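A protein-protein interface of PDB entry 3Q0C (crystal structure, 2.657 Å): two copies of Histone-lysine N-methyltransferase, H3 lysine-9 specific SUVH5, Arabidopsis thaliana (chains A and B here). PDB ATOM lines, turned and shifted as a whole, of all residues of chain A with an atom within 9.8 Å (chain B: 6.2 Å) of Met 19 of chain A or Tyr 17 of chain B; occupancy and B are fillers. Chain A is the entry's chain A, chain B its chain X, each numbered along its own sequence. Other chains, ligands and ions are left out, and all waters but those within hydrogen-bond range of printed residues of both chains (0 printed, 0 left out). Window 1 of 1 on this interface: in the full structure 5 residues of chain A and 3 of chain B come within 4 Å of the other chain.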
ATOM      1  N   PHE A  15     -10.427  15.832  21.230  1.00  0.00           N
ATOM      2  CA  PHE A  15     -10.628  17.263  21.442  1.00  0.00           C
ATOM      3  C   PHE A  15     -11.993  17.702  20.946  1.00  0.00           C
ATOM      4  O   PHE A  15     -12.544  17.116  20.020  1.00  0.00           O
ATOM      5  CB  PHE A  15      -9.540  18.069  20.736  1.00  0.00           C
ATOM      6  CG  PHE A  15      -8.166  17.523  20.949  1.00  0.00           C
ATOM      7  CD1 PHE A  15      -7.390  17.961  22.002  1.00  0.00           C
ATOM      8  CD2 PHE A  15      -7.657  16.548  20.107  1.00  0.00           C
ATOM      9  CE1 PHE A  15      -6.124  17.446  22.206  1.00  0.00           C
ATOM     10  CE2 PHE A  15      -6.395  16.029  20.306  1.00  0.00           C
ATOM     11  CZ  PHE A  15      -5.626  16.480  21.356  1.00  0.00           C
ATOM     12  N   GLN A  16     -12.527  18.756  21.552  1.00  0.00           N
ATOM     13  CA  GLN A  16     -13.858  19.243  21.216  1.00  0.00           C
ATOM     14  C   GLN A  16     -13.846  20.378  20.176  1.00  0.00           C
ATOM     15  O   GLN A  16     -14.765  20.493  19.362  1.00  0.00           O
ATOM     16  CB  GLN A  16     -14.556  19.694  22.494  1.00  0.00           C
ATOM     17  CG  GLN A  16     -16.030  19.994  22.364  1.00  0.00           C
ATOM     18  CD  GLN A  16     -16.549  20.734  23.583  1.00  0.00           C
ATOM     19  OE1 GLN A  16     -17.739  21.036  23.686  1.00  0.00           O
ATOM     20  NE2 GLN A  16     -15.648  21.037  24.516  1.00  0.00           N
ATOM     21  N   TYR A  17     -12.797  21.199  20.194  1.00  0.00           N
ATOM     22  CA  TYR A  17     -12.762  22.401  19.366  1.00  0.00           C
ATOM     23  C   TYR A  17     -11.438  22.606  18.650  1.00  0.00           C
ATOM     24  O   TYR A  17     -10.373  22.304  19.184  1.00  0.00           O
ATOM     25  CB  TYR A  17     -13.092  23.652  20.200  1.00  0.00           C
ATOM     26  CG  TYR A  17     -14.526  23.701  20.687  1.00  0.00           C
ATOM     27  CD1 TYR A  17     -15.580  23.824  19.787  1.00  0.00           C
ATOM     28  CD2 TYR A  17     -14.829  23.614  22.043  1.00  0.00           C
ATOM     29  CE1 TYR A  17     -16.893  23.859  20.218  1.00  0.00           C
ATOM     30  CE2 TYR A  17     -16.144  23.656  22.488  1.00  0.00           C
ATOM     31  CZ  TYR A  17     -17.169  23.777  21.568  1.00  0.00           C
ATOM     32  OH  TYR A  17     -18.475  23.822  21.993  1.00  0.00           O
ATOM     33  N   ARG A  18     -11.535  23.132  17.431  1.00  0.00           N
ATOM     34  CA  ARG A  18     -10.384  23.482  16.606  1.00  0.00           C
ATOM     35  C   ARG A  18      -9.343  24.288  17.373  1.00  0.00           C
ATOM     36  O   ARG A  18      -8.135  24.181  17.124  1.00  0.00           O
ATOM     37  CB  ARG A  18     -10.847  24.278  15.381  1.00  0.00           C
ATOM     38  CG  ARG A  18     -11.672  23.461  14.410  1.00  0.00           C
ATOM     39  CD  ARG A  18     -10.834  22.333  13.854  1.00  0.00           C
ATOM     40  NE  ARG A  18      -9.613  22.870  13.272  1.00  0.00           N
ATOM     41  CZ  ARG A  18      -9.485  23.179  11.988  1.00  0.00           C
ATOM     42  NH1 ARG A  18     -10.497  22.978  11.150  1.00  0.00           N
ATOM     43  NH2 ARG A  18      -8.345  23.680  11.548  1.00  0.00           N
ATOM     44  N   MET A  19      -9.817  25.100  18.309  1.00  0.00           N
ATOM     45  CA  MET A  19      -8.921  25.971  19.054  1.00  0.00           C
ATOM     46  C   MET A  19      -8.103  25.211  20.108  1.00  0.00           C
ATOM     47  O   MET A  19      -6.994  25.625  20.447  1.00  0.00           O
ATOM     48  CB  MET A  19      -9.687  27.148  19.672  1.00  0.00           C
ATOM     49  CG  MET A  19     -10.009  28.296  18.693  1.00  0.00           C
ATOM     50  SD  MET A  19      -8.562  29.177  18.020  1.00  0.00           S
ATOM     51  CE  MET A  19      -8.461  28.408  16.416  1.00  0.00           C
ATOM     52  N   GLU A  20      -8.640  24.104  20.618  1.00  0.00           N
ATOM     53  CA  GLU A  20      -7.865  23.245  21.510  1.00  0.00           C
ATOM     54  C   GLU A  20      -6.623  22.740  20.791  1.00  0.00           C
ATOM     55  O   GLU A  20      -5.559  22.614  21.394  1.00  0.00           O
ATOM     56  CB  GLU A  20      -8.687  22.051  21.984  1.00  0.00           C
ATOM     57  CG  GLU A  20      -9.965  22.404  22.701  1.00  0.00           C
ATOM     58  CD  GLU A  20     -10.691  21.171  23.210  1.00  0.00           C
ATOM     59  OE1 GLU A  20     -10.137  20.443  24.067  1.00  0.00           O
ATOM     60  OE2 GLU A  20     -11.821  20.925  22.749  1.00  0.00           O
ATOM     61  N   LEU A  21      -6.767  22.445  19.499  1.00  0.00           N
ATOM     62  CA  LEU A  21      -5.645  21.987  18.688  1.00  0.00           C
ATOM     63  C   LEU A  21      -4.621  23.094  18.572  1.00  0.00           C
ATOM     64  O   LEU A  21      -3.414  22.860  18.641  1.00  0.00           O
ATOM     65  CB  LEU A  21      -6.116  21.600  17.292  1.00  0.00           C
ATOM     66  CG  LEU A  21      -7.231  20.562  17.242  1.00  0.00           C
ATOM     67  CD1 LEU A  21      -7.696  20.365  15.804  1.00  0.00           C
ATOM     68  CD2 LEU A  21      -6.762  19.255  17.859  1.00  0.00           C
ATOM     69  N   ASN A  22      -5.117  24.308  18.379  1.00  0.00           N
ATOM     70  CA  ASN A  22      -4.260  25.483  18.318  1.00  0.00           C
ATOM     71  C   ASN A  22      -3.489  25.661  19.626  1.00  0.00           C
ATOM     72  O   ASN A  22      -2.271  25.859  19.621  1.00  0.00           O
ATOM     73  CB  ASN A  22      -5.091  26.732  17.996  1.00  0.00           C
ATOM     74  CG  ASN A  22      -4.279  28.013  18.054  1.00  0.00           C
ATOM     75  OD1 ASN A  22      -3.775  28.397  19.109  1.00  0.00           O
ATOM     76  ND2 ASN A  22      -4.164  28.691  16.918  1.00  0.00           N
ATOM     77  N   LEU A  23      -4.207  25.574  20.742  1.00  0.00           N
ATOM     78  CA  LEU A  23      -3.595  25.733  22.053  1.00  0.00           C
ATOM     79  C   LEU A  23      -2.434  24.767  22.253  1.00  0.00           C
ATOM     80  O   LEU A  23      -1.337  25.175  22.643  1.00  0.00           O
ATOM     81  CB  LEU A  23      -4.642  25.558  23.157  1.00  0.00           C
ATOM     82  CG  LEU A  23      -5.288  26.859  23.665  1.00  0.00           C
ATOM     83  CD1 LEU A  23      -4.964  28.058  22.761  1.00  0.00           C
ATOM     84  CD2 LEU A  23      -6.805  26.699  23.882  1.00  0.00           C
ATOM     85  N   LEU A  24      -2.672  23.491  21.963  1.00  0.00           N
ATOM     86  CA  LEU A  24      -1.652  22.468  22.160  1.00  0.00           C
ATOM     87  C   LEU A  24      -0.533  22.510  21.113  1.00  0.00           C
ATOM     88  O   LEU A  24       0.498  21.853  21.276  1.00  0.00           O
ATOM     89  CB  LEU A  24      -2.290  21.080  22.233  1.00  0.00           C
ATOM     90  CG  LEU A  24      -3.283  20.931  23.388  1.00  0.00           C
ATOM     91  CD1 LEU A  24      -3.882  19.536  23.435  1.00  0.00           C
ATOM     92  CD2 LEU A  24      -2.607  21.264  24.707  1.00  0.00           C
ATOM     93  N   GLY A  25      -0.727  23.294  20.055  1.00  0.00           N
ATOM     94  CA  GLY A  25       0.280  23.424  19.010  1.00  0.00           C
ATOM     95  C   GLY A  25       0.166  22.326  17.962  1.00  0.00           C
ATOM     96  O   GLY A  25       1.044  22.150  17.105  1.00  0.00           O
ATOM     97  N   ILE A  26      -0.935  21.584  18.044  1.00  0.00           N
ATOM     98  CA  ILE A  26      -1.233  20.498  17.126  1.00  0.00           C
ATOM     99  C   ILE A  26      -1.519  21.015  15.715  1.00  0.00           C
ATOM    100  O   ILE A  26      -0.896  20.588  14.735  1.00  0.00           O
ATOM    101  CB  ILE A  26      -2.468  19.732  17.613  1.00  0.00           C
ATOM    102  CG1 ILE A  26      -2.174  19.067  18.960  1.00  0.00           C
ATOM    103  CG2 ILE A  26      -2.922  18.727  16.564  1.00  0.00           C
ATOM    104  CD1 ILE A  26      -3.388  18.459  19.618  1.00  0.00           C
ATOM    105  N   HIS A  27      -2.471  21.938  15.630  1.00  0.00           N
ATOM    106  CA  HIS A  27      -2.901  22.495  14.360  1.00  0.00           C
ATOM    107  C   HIS A  27      -3.306  23.944  14.597  1.00  0.00           C
ATOM    108  O   HIS A  27      -4.214  24.221  15.390  1.00  0.00           O
ATOM    109  CB  HIS A  27      -4.080  21.685  13.802  1.00  0.00           C
ATOM    110  CG  HIS A  27      -4.361  21.942  12.354  1.00  0.00           C
ATOM    111  ND1 HIS A  27      -5.499  22.590  11.919  1.00  0.00           N
ATOM    112  CD2 HIS A  27      -3.642  21.655  11.243  1.00  0.00           C
ATOM    113  CE1 HIS A  27      -5.472  22.687  10.601  1.00  0.00           C
ATOM    114  NE2 HIS A  27      -4.355  22.129  10.165  1.00  0.00           N
ATOM    115  N   ARG A  28      -2.640  24.867  13.911  1.00  0.00           N
ATOM    116  CA  ARG A  28      -2.834  26.292  14.183  1.00  0.00           C
ATOM    117  C   ARG A  28      -4.112  26.910  13.603  1.00  0.00           C
ATOM    118  O   ARG A  28      -4.842  27.596  14.316  1.00  0.00           O
ATOM    119  CB  ARG A  28      -1.603  27.108  13.766  1.00  0.00           C
ATOM    120  CG  ARG A  28      -0.366  26.829  14.612  1.00  0.00           C
ATOM    121  CD  ARG A  28       0.760  27.769  14.221  1.00  0.00           C
ATOM    122  NE  ARG A  28       0.904  27.850  12.769  1.00  0.00           N
ATOM    123  CZ  ARG A  28       1.505  28.850  12.130  1.00  0.00           C
ATOM    124  NH1 ARG A  28       2.014  29.870  12.816  1.00  0.00           N
ATOM    125  NH2 ARG A  28       1.589  28.842  10.803  1.00  0.00           N
ATOM    126  N   PRO A  29      -4.390  26.678  12.313  1.00  0.00           N
ATOM    127  CA  PRO A  29      -5.539  27.367  11.714  1.00  0.00           C
ATOM    128  C   PRO A  29      -6.856  27.130  12.456  1.00  0.00           C
ATOM    129  O   PRO A  29      -7.125  26.048  12.990  1.00  0.00           O
ATOM    130  CB  PRO A  29      -5.595  26.790  10.296  1.00  0.00           C
ATOM    131  CG  PRO A  29      -4.182  26.402  10.010  1.00  0.00           C
ATOM    132  CD  PRO A  29      -3.637  25.894  11.322  1.00  0.00           C
ATOM    133  N   SER A  30      -7.671  28.173  12.490  1.00  0.00           N
ATOM    134  CA  SER A  30      -8.961  28.118  13.151  1.00  0.00           C
ATOM    135  C   SER A  30      -9.948  27.357  12.285  1.00  0.00           C
ATOM    136  O   SER A  30     -10.873  26.719  12.790  1.00  0.00           O
ATOM    137  CB  SER A  30      -9.480  29.540  13.397  1.00  0.00           C
ATOM    138  OG  SER A  30      -9.511  30.293  12.193  1.00  0.00           O
ATOM    139  N   GLN A  31      -9.733  27.425  10.976  1.00  0.00           N
ATOM    140  CA  GLN A  31     -10.734  26.984  10.012  1.00  0.00           C
ATOM    141  C   GLN A  31     -10.104  26.138   8.896  1.00  0.00           C
ATOM    142  O   GLN A  31     -10.608  25.069   8.536  1.00  0.00           O
ATOM    143  CB  GLN A  31     -11.423  28.217   9.423  1.00  0.00           C
ATOM    144  CG  GLN A  31     -12.815  27.992   8.891  1.00  0.00           C
ATOM    145  CD  GLN A  31     -13.573  29.290   8.741  1.00  0.00           C
ATOM    146  OE1 GLN A  31     -13.474  30.183   9.588  1.00  0.00           O
ATOM    147  NE2 GLN A  31     -14.338  29.408   7.663  1.00  0.00           N
ATOM    148  N   SER A  32      -8.991  26.628   8.362  1.00  0.00           N
ATOM    149  CA  SER A  32      -8.304  25.965   7.262  1.00  0.00           C
ATOM    150  C   SER A  32      -7.917  24.529   7.612  1.00  0.00           C
ATOM    151  O   SER A  32      -7.495  24.248   8.735  1.00  0.00           O
ATOM    152  CB  SER A  32      -7.058  26.762   6.864  1.00  0.00           C
ATOM    153  OG  SER A  32      -6.299  26.083   5.882  1.00  0.00           O
ATOM    154  N   VAL A  50      -6.450  18.496   8.728  1.00  0.00           N
ATOM    155  CA  VAL A  50      -7.683  18.073   9.374  1.00  0.00           C
ATOM    156  C   VAL A  50      -8.645  17.516   8.337  1.00  0.00           C
ATOM    157  O   VAL A  50      -8.910  18.144   7.310  1.00  0.00           O
ATOM    158  CB  VAL A  50      -8.392  19.248  10.097  1.00  0.00           C
ATOM    159  CG1 VAL A  50      -9.631  18.745  10.833  1.00  0.00           C
ATOM    160  CG2 VAL A  50      -7.446  19.958  11.047  1.00  0.00           C
ATOM    161  N   ILE A 108      -5.226  15.010  11.859  1.00  0.00           N
ATOM    162  CA  ILE A 108      -6.331  15.054  12.807  1.00  0.00           C
ATOM    163  C   ILE A 108      -7.631  14.724  12.091  1.00  0.00           C
ATOM    164  O   ILE A 108      -8.000  15.376  11.114  1.00  0.00           O
ATOM    165  CB  ILE A 108      -6.471  16.445  13.463  1.00  0.00           C
ATOM    166  CG1 ILE A 108      -5.193  16.817  14.219  1.00  0.00           C
ATOM    167  CG2 ILE A 108      -7.671  16.463  14.378  1.00  0.00           C
ATOM    168  CD1 ILE A 108      -4.104  17.448  13.346  1.00  0.00           C
ATOM    169  N   LYS A 123     -16.489  15.628  22.045  1.00  0.00           N
ATOM    170  CA  LYS A 123     -15.316  15.055  21.387  1.00  0.00           C
ATOM    171  C   LYS A 123     -15.517  14.896  19.874  1.00  0.00           C
ATOM    172  O   LYS A 123     -16.175  13.957  19.411  1.00  0.00           O
ATOM    173  CB  LYS A 123     -14.940  13.719  22.035  1.00  0.00           C
ATOM    174  CG  LYS A 123     -13.815  13.813  23.060  1.00  0.00           C
ATOM    175  CD  LYS A 123     -13.766  15.171  23.740  1.00  0.00           C
ATOM    176  CE  LYS A 123     -12.666  15.211  24.794  1.00  0.00           C
ATOM    177  NZ  LYS A 123     -12.320  16.606  25.200  1.00  0.00           N
ATOM    178  N   TYR A 125     -12.730  15.565  17.497  1.00  0.00           N
ATOM    179  CA  TYR A 125     -11.474  15.351  16.789  1.00  0.00           C
ATOM    180  C   TYR A 125     -10.550  14.368  17.502  1.00  0.00           C
ATOM    181  O   TYR A 125     -10.430  14.413  18.721  1.00  0.00           O
ATOM    182  CB  TYR A 125     -10.747  16.678  16.627  1.00  0.00           C
ATOM    183  CG  TYR A 125     -11.513  17.723  15.851  1.00  0.00           C
ATOM    184  CD1 TYR A 125     -11.490  17.734  14.463  1.00  0.00           C
ATOM    185  CD2 TYR A 125     -12.242  18.715  16.506  1.00  0.00           C
ATOM    186  CE1 TYR A 125     -12.177  18.694  13.743  1.00  0.00           C
ATOM    187  CE2 TYR A 125     -12.936  19.687  15.791  1.00  0.00           C
ATOM    188  CZ  TYR A 125     -12.899  19.668  14.409  1.00  0.00           C
ATOM    189  OH  TYR A 125     -13.575  20.620  13.683  1.00  0.00           O
ATOM    190  N   PHE B  15      -9.127  35.086  28.992  1.00  0.00           N
ATOM    191  CA  PHE B  15      -9.507  33.942  28.164  1.00  0.00           C
ATOM    192  C   PHE B  15      -9.022  34.110  26.730  1.00  0.00           C
ATOM    193  O   PHE B  15      -8.989  35.222  26.204  1.00  0.00           O
ATOM    194  CB  PHE B  15     -11.024  33.738  28.195  1.00  0.00           C
ATOM    195  CG  PHE B  15     -11.606  33.810  29.568  1.00  0.00           C
ATOM    196  CD1 PHE B  15     -11.732  32.674  30.338  1.00  0.00           C
ATOM    197  CD2 PHE B  15     -12.001  35.021  30.100  1.00  0.00           C
ATOM    198  CE1 PHE B  15     -12.253  32.743  31.610  1.00  0.00           C
ATOM    199  CE2 PHE B  15     -12.520  35.097  31.372  1.00  0.00           C
ATOM    200  CZ  PHE B  15     -12.648  33.958  32.127  1.00  0.00           C
ATOM    201  N   GLN B  16      -8.639  32.994  26.115  1.00  0.00           N
ATOM    202  CA  GLN B  16      -8.060  32.999  24.775  1.00  0.00           C
ATOM    203  C   GLN B  16      -9.135  33.023  23.693  1.00  0.00           C
ATOM    204  O   GLN B  16      -8.958  33.659  22.653  1.00  0.00           O
ATOM    205  CB  GLN B  16      -7.132  31.789  24.584  1.00  0.00           C
ATOM    206  CG  GLN B  16      -6.143  31.899  23.407  1.00  0.00           C
ATOM    207  CD  GLN B  16      -6.603  31.189  22.120  1.00  0.00           C
ATOM    208  OE1 GLN B  16      -5.803  30.964  21.205  1.00  0.00           O
ATOM    209  NE2 GLN B  16      -7.883  30.836  22.050  1.00  0.00           N
ATOM    210  N   TYR B  17     -10.250  32.338  23.926  1.00  0.00           N
ATOM    211  CA  TYR B  17     -11.291  32.289  22.907  1.00  0.00           C
ATOM    212  C   TYR B  17     -12.731  32.166  23.447  1.00  0.00           C
ATOM    213  O   TYR B  17     -12.957  31.713  24.571  1.00  0.00           O
ATOM    214  CB  TYR B  17     -10.963  31.207  21.862  1.00  0.00           C
ATOM    215  CG  TYR B  17     -11.044  29.775  22.354  1.00  0.00           C
ATOM    216  CD1 TYR B  17      -9.901  29.060  22.703  1.00  0.00           C
ATOM    217  CD2 TYR B  17     -12.273  29.126  22.447  1.00  0.00           C
ATOM    218  CE1 TYR B  17      -9.987  27.736  23.144  1.00  0.00           C
ATOM    219  CE2 TYR B  17     -12.368  27.812  22.887  1.00  0.00           C
ATOM    220  CZ  TYR B  17     -11.231  27.124  23.231  1.00  0.00           C
ATOM    221  OH  TYR B  17     -11.364  25.826  23.667  1.00  0.00           O
ATOM    222  N   ARG B  18     -13.692  32.567  22.617  1.00  0.00           N
ATOM    223  CA  ARG B  18     -15.105  32.694  22.997  1.00  0.00           C
ATOM    224  C   ARG B  18     -15.787  31.447  23.591  1.00  0.00           C
ATOM    225  O   ARG B  18     -16.655  31.574  24.453  1.00  0.00           O
ATOM    226  CB  ARG B  18     -15.929  33.215  21.811  1.00  0.00           C
ATOM    227  CG  ARG B  18     -15.613  34.645  21.396  1.00  0.00           C
ATOM    228  CD  ARG B  18     -16.456  35.640  22.170  1.00  0.00           C
ATOM    229  NE  ARG B  18     -17.872  35.285  22.135  1.00  0.00           N
ATOM    230  CZ  ARG B  18     -18.791  35.936  21.429  1.00  0.00           C
ATOM    231  NH1 ARG B  18     -18.459  36.998  20.705  1.00  0.00           N
ATOM    232  NH2 ARG B  18     -20.048  35.525  21.455  1.00  0.00           N
ATOM    233  N   MET B  19     -15.417  30.255  23.132  1.00  0.00           N
ATOM    234  CA  MET B  19     -16.036  29.031  23.644  1.00  0.00           C
ATOM    235  C   MET B  19     -15.638  28.747  25.094  1.00  0.00           C
ATOM    236  O   MET B  19     -16.359  28.064  25.821  1.00  0.00           O
ATOM    237  CB  MET B  19     -15.727  27.831  22.740  1.00  0.00           C
ATOM    238  CG  MET B  19     -16.567  27.753  21.462  1.00  0.00           C
ATOM    239  SD  MET B  19     -18.316  27.444  21.759  1.00  0.00           S
ATOM    240  CE  MET B  19     -18.971  29.081  21.565  1.00  0.00           C
ATOM    241  N   GLU B  20     -14.491  29.272  25.513  1.00  0.00           N
ATOM    242  CA  GLU B  20     -14.103  29.197  26.919  1.00  0.00           C
ATOM    243  C   GLU B  20     -15.121  29.928  27.786  1.00  0.00           C
ATOM    244  O   GLU B  20     -15.425  29.498  28.896  1.00  0.00           O
ATOM    245  CB  GLU B  20     -12.727  29.816  27.142  1.00  0.00           C
ATOM    246  CG  GLU B  20     -11.612  29.191  26.348  1.00  0.00           C
ATOM    247  CD  GLU B  20     -10.276  29.812  26.682  1.00  0.00           C
ATOM    248  OE1 GLU B  20      -9.804  29.644  27.829  1.00  0.00           O
ATOM    249  OE2 GLU B  20      -9.701  30.482  25.802  1.00  0.00           O
ATOM    250  N   LEU B  21     -15.633  31.043  27.274  1.00  0.00           N
ATOM    251  CA  LEU B  21     -16.640  31.819  27.980  1.00  0.00           C
ATOM    252  C   LEU B  21     -17.903  30.999  28.105  1.00  0.00           C
ATOM    253  O   LEU B  21     -18.564  31.002  29.142  1.00  0.00           O
ATOM    254  CB  LEU B  21     -16.945  33.104  27.224  1.00  0.00           C
ATOM    255  CG  LEU B  21     -15.748  33.995  26.916  1.00  0.00           C
ATOM    256  CD1 LEU B  21     -16.169  35.177  26.063  1.00  0.00           C
ATOM    257  CD2 LEU B  21     -15.095  34.462  28.201  1.00  0.00           C
ATOM    258  N   ASN B  22     -18.231  30.298  27.029  1.00  0.00           N
ATOM    259  CA  ASN B  22     -19.388  29.426  27.006  1.00  0.00           C
ATOM    260  C   ASN B  22     -19.241  28.330  28.043  1.00  0.00           C
ATOM    261  O   ASN B  22     -20.162  28.067  28.813  1.00  0.00           O
ATOM    262  CB  ASN B  22     -19.579  28.830  25.604  1.00  0.00           C
ATOM    263  CG  ASN B  22     -20.688  27.799  25.549  1.00  0.00           C
ATOM    264  OD1 ASN B  22     -20.591  26.733  26.154  1.00  0.00           O
ATOM    265  ND2 ASN B  22     -21.743  28.106  24.809  1.00  0.00           N
ATOM    266  N   LEU B  23     -18.071  27.702  28.060  1.00  0.00           N
ATOM    267  CA  LEU B  23     -17.799  26.618  28.996  1.00  0.00           C
ATOM    268  C   LEU B  23     -18.007  27.046  30.443  1.00  0.00           C
ATOM    269  O   LEU B  23     -18.704  26.374  31.202  1.00  0.00           O
ATOM    270  CB  LEU B  23     -16.384  26.081  28.790  1.00  0.00           C
ATOM    271  CG  LEU B  23     -16.261  24.862  27.861  1.00  0.00           C
ATOM    272  CD1 LEU B  23     -17.547  24.587  27.079  1.00  0.00           C
ATOM    273  CD2 LEU B  23     -15.054  24.985  26.921  1.00  0.00           C
ATOM    274  N   ASN B 124      -7.279  36.865  24.563  1.00  0.00           N
ATOM    275  CA  ASN B 124      -7.991  37.846  23.746  1.00  0.00           C
ATOM    276  C   ASN B 124      -9.193  38.489  24.440  1.00  0.00           C
ATOM    277  O   ASN B 124      -9.753  39.462  23.943  1.00  0.00           O
ATOM    278  CB  ASN B 124      -8.422  37.215  22.415  1.00  0.00           C
ATOM    279  CG  ASN B 124      -7.239  36.837  21.535  1.00  0.00           C
ATOM    280  OD1 ASN B 124      -6.820  35.679  21.507  1.00  0.00           O
ATOM    281  ND2 ASN B 124      -6.692  37.816  20.816  1.00  0.00           N
ATOM    282  N   TYR B 125      -9.576  37.958  25.594  1.00  0.00           N
ATOM    283  CA  TYR B 125     -10.727  38.482  26.314  1.00  0.00           C
ATOM    284  C   TYR B 125     -10.477  38.603  27.820  1.00  0.00           C
ATOM    285  O   TYR B 125      -9.856  37.725  28.423  1.00  0.00           O
ATOM    286  CB  TYR B 125     -11.936  37.576  26.078  1.00  0.00           C
ATOM    287  CG  TYR B 125     -12.359  37.432  24.633  1.00  0.00           C
ATOM    288  CD1 TYR B 125     -13.178  38.378  24.038  1.00  0.00           C
ATOM    289  CD2 TYR B 125     -11.965  36.332  23.873  1.00  0.00           C
ATOM    290  CE1 TYR B 125     -13.581  38.247  22.732  1.00  0.00           C
ATOM    291  CE2 TYR B 125     -12.367  36.194  22.561  1.00  0.00           C
ATOM    292  CZ  TYR B 125     -13.176  37.158  21.996  1.00  0.00           C
ATOM    293  OH  TYR B 125     -13.596  37.055  20.690  1.00  0.00           O
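Of the 22 printed residues of chain A, 5 touch a printed residue of chain B. Hydrophobic or aromatic side chains of chain A that line the printed part of chain B: Tyr 17, Met 19 and Leu 23. Among the printed residues, 6 pairs touch across the chains. Among the printed residues, no Asp or Glu carboxylate lies within 4 Å of a Lys or Arg side-chain nitrogen of the other chain.
Of the printed residues of chain B, Tyr 17 of chain A touches Met 19 (3.6 Å). Of chain B, only Tyr 17 (3.5 Å) comes within 4 Å of Met 19 of chain A. Of the printed residues of chain B, Asn 22 of chain A touches Gln 16. Of the printed residues of chain B, Leu 23 of chain A touches Gln 16 (3.4 Å) and Tyr 17 (3.4 Å). Gln 31 of chain A touches none of the printed residues of chain B. Of chain A, only Asn 22 and Leu 23 come within 4 Å of Gln 16 of chain B. Of chain A, only Met 19 (3.5 Å), Glu 20 (3.8 Å) and Leu 23 (3.4 Å) come within 4 Å of Tyr 17 of chain B. Glu 20 of chain B touches none of the printed residues of chain A. The nearest residue of chain A that does not touch Tyr 17 of chain B is Tyr 17 of chain A (4.4 Å). The nearest printed residue of chain B that does not touch Glu 20 of chain A is Leu 23 of chain B (6.7 Å).
The side-chain carboxylate (OE2) of Glu 20 of chain B is in hydrogen-bond range of the backbone NH (N) of Gln 16 of chain B. O of Gln 16 of chain B sits close to OD1 of Asn 124 of chain B (3.2 Å). The side-chain amide oxygen (OE1) of Gln 16 of chain A lies close to the side-chain hydroxyl (OH) of Tyr 17 of chain A (3.3 Å). The backbone NH (N) of Gln 16 of chain A is in hydrogen-bond range of the side-chain carboxylate (OE2) of Glu 20 of chain A (2.6 Å). The backbone NH (N) of Tyr 17 of chain A sits at hydrogen-bond distance from the side-chain carboxylate (OE2) of Glu 20 of chain A (2.7 Å). The side-chain amide nitrogen of Asn 22 of chain A lies within hydrogen-bond range of the backbone carbonyl oxygen of Arg 28 of chain A.
The side-chain hydroxyl (OH) of Tyr 17 of chain A lies within hydrogen-bond range of the side-chain sulfur (SD) of Met 19 of chain B, at 3.6 Å.
Glu 20 of chain A touches Tyr 17 of chain B, but with the chains exchanged Tyr 17 of chain A does not touch Glu 20 of chain B (6.6 Å). Asn 22 of chain A touches Gln 16 of chain B, but with the chains exchanged Gln 16 of chain A does not touch Asn 22 of chain B (6.8 Å). Leu 23 of chain A touches Gln 16 of chain B, but with the chains exchanged Gln 16 of chain A does not touch Leu 23 of chain B (4.7 Å). Leu 23 of chain A touches Tyr 17 of chain B, but with the chains exchanged Tyr 17 of chain A does not touch Leu 23 of chain B (4.8 Å). Positions printed for both chains: 15, 16, 17, 18, 19, 20, 21, 22, 23 and 125. Of the 6 pairs that touch across the chains among the printed residues, 2 have their exchanged pair printed and touching as well.
Among the printed residues, merely in contact across the chains: Leu 23 of chain A with Gln 16 of chain B (3.4 Å), Leu 23 of chain A with Tyr 17 of chain B (3.4 Å), Met 19 of chain A with Tyr 17 of chain B (3.5 Å), Glu 20 of chain A with Tyr 17 of chain B (3.8 Å) and Asn 22 of chain A with Gln 16 of chain B (3.9 Å).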
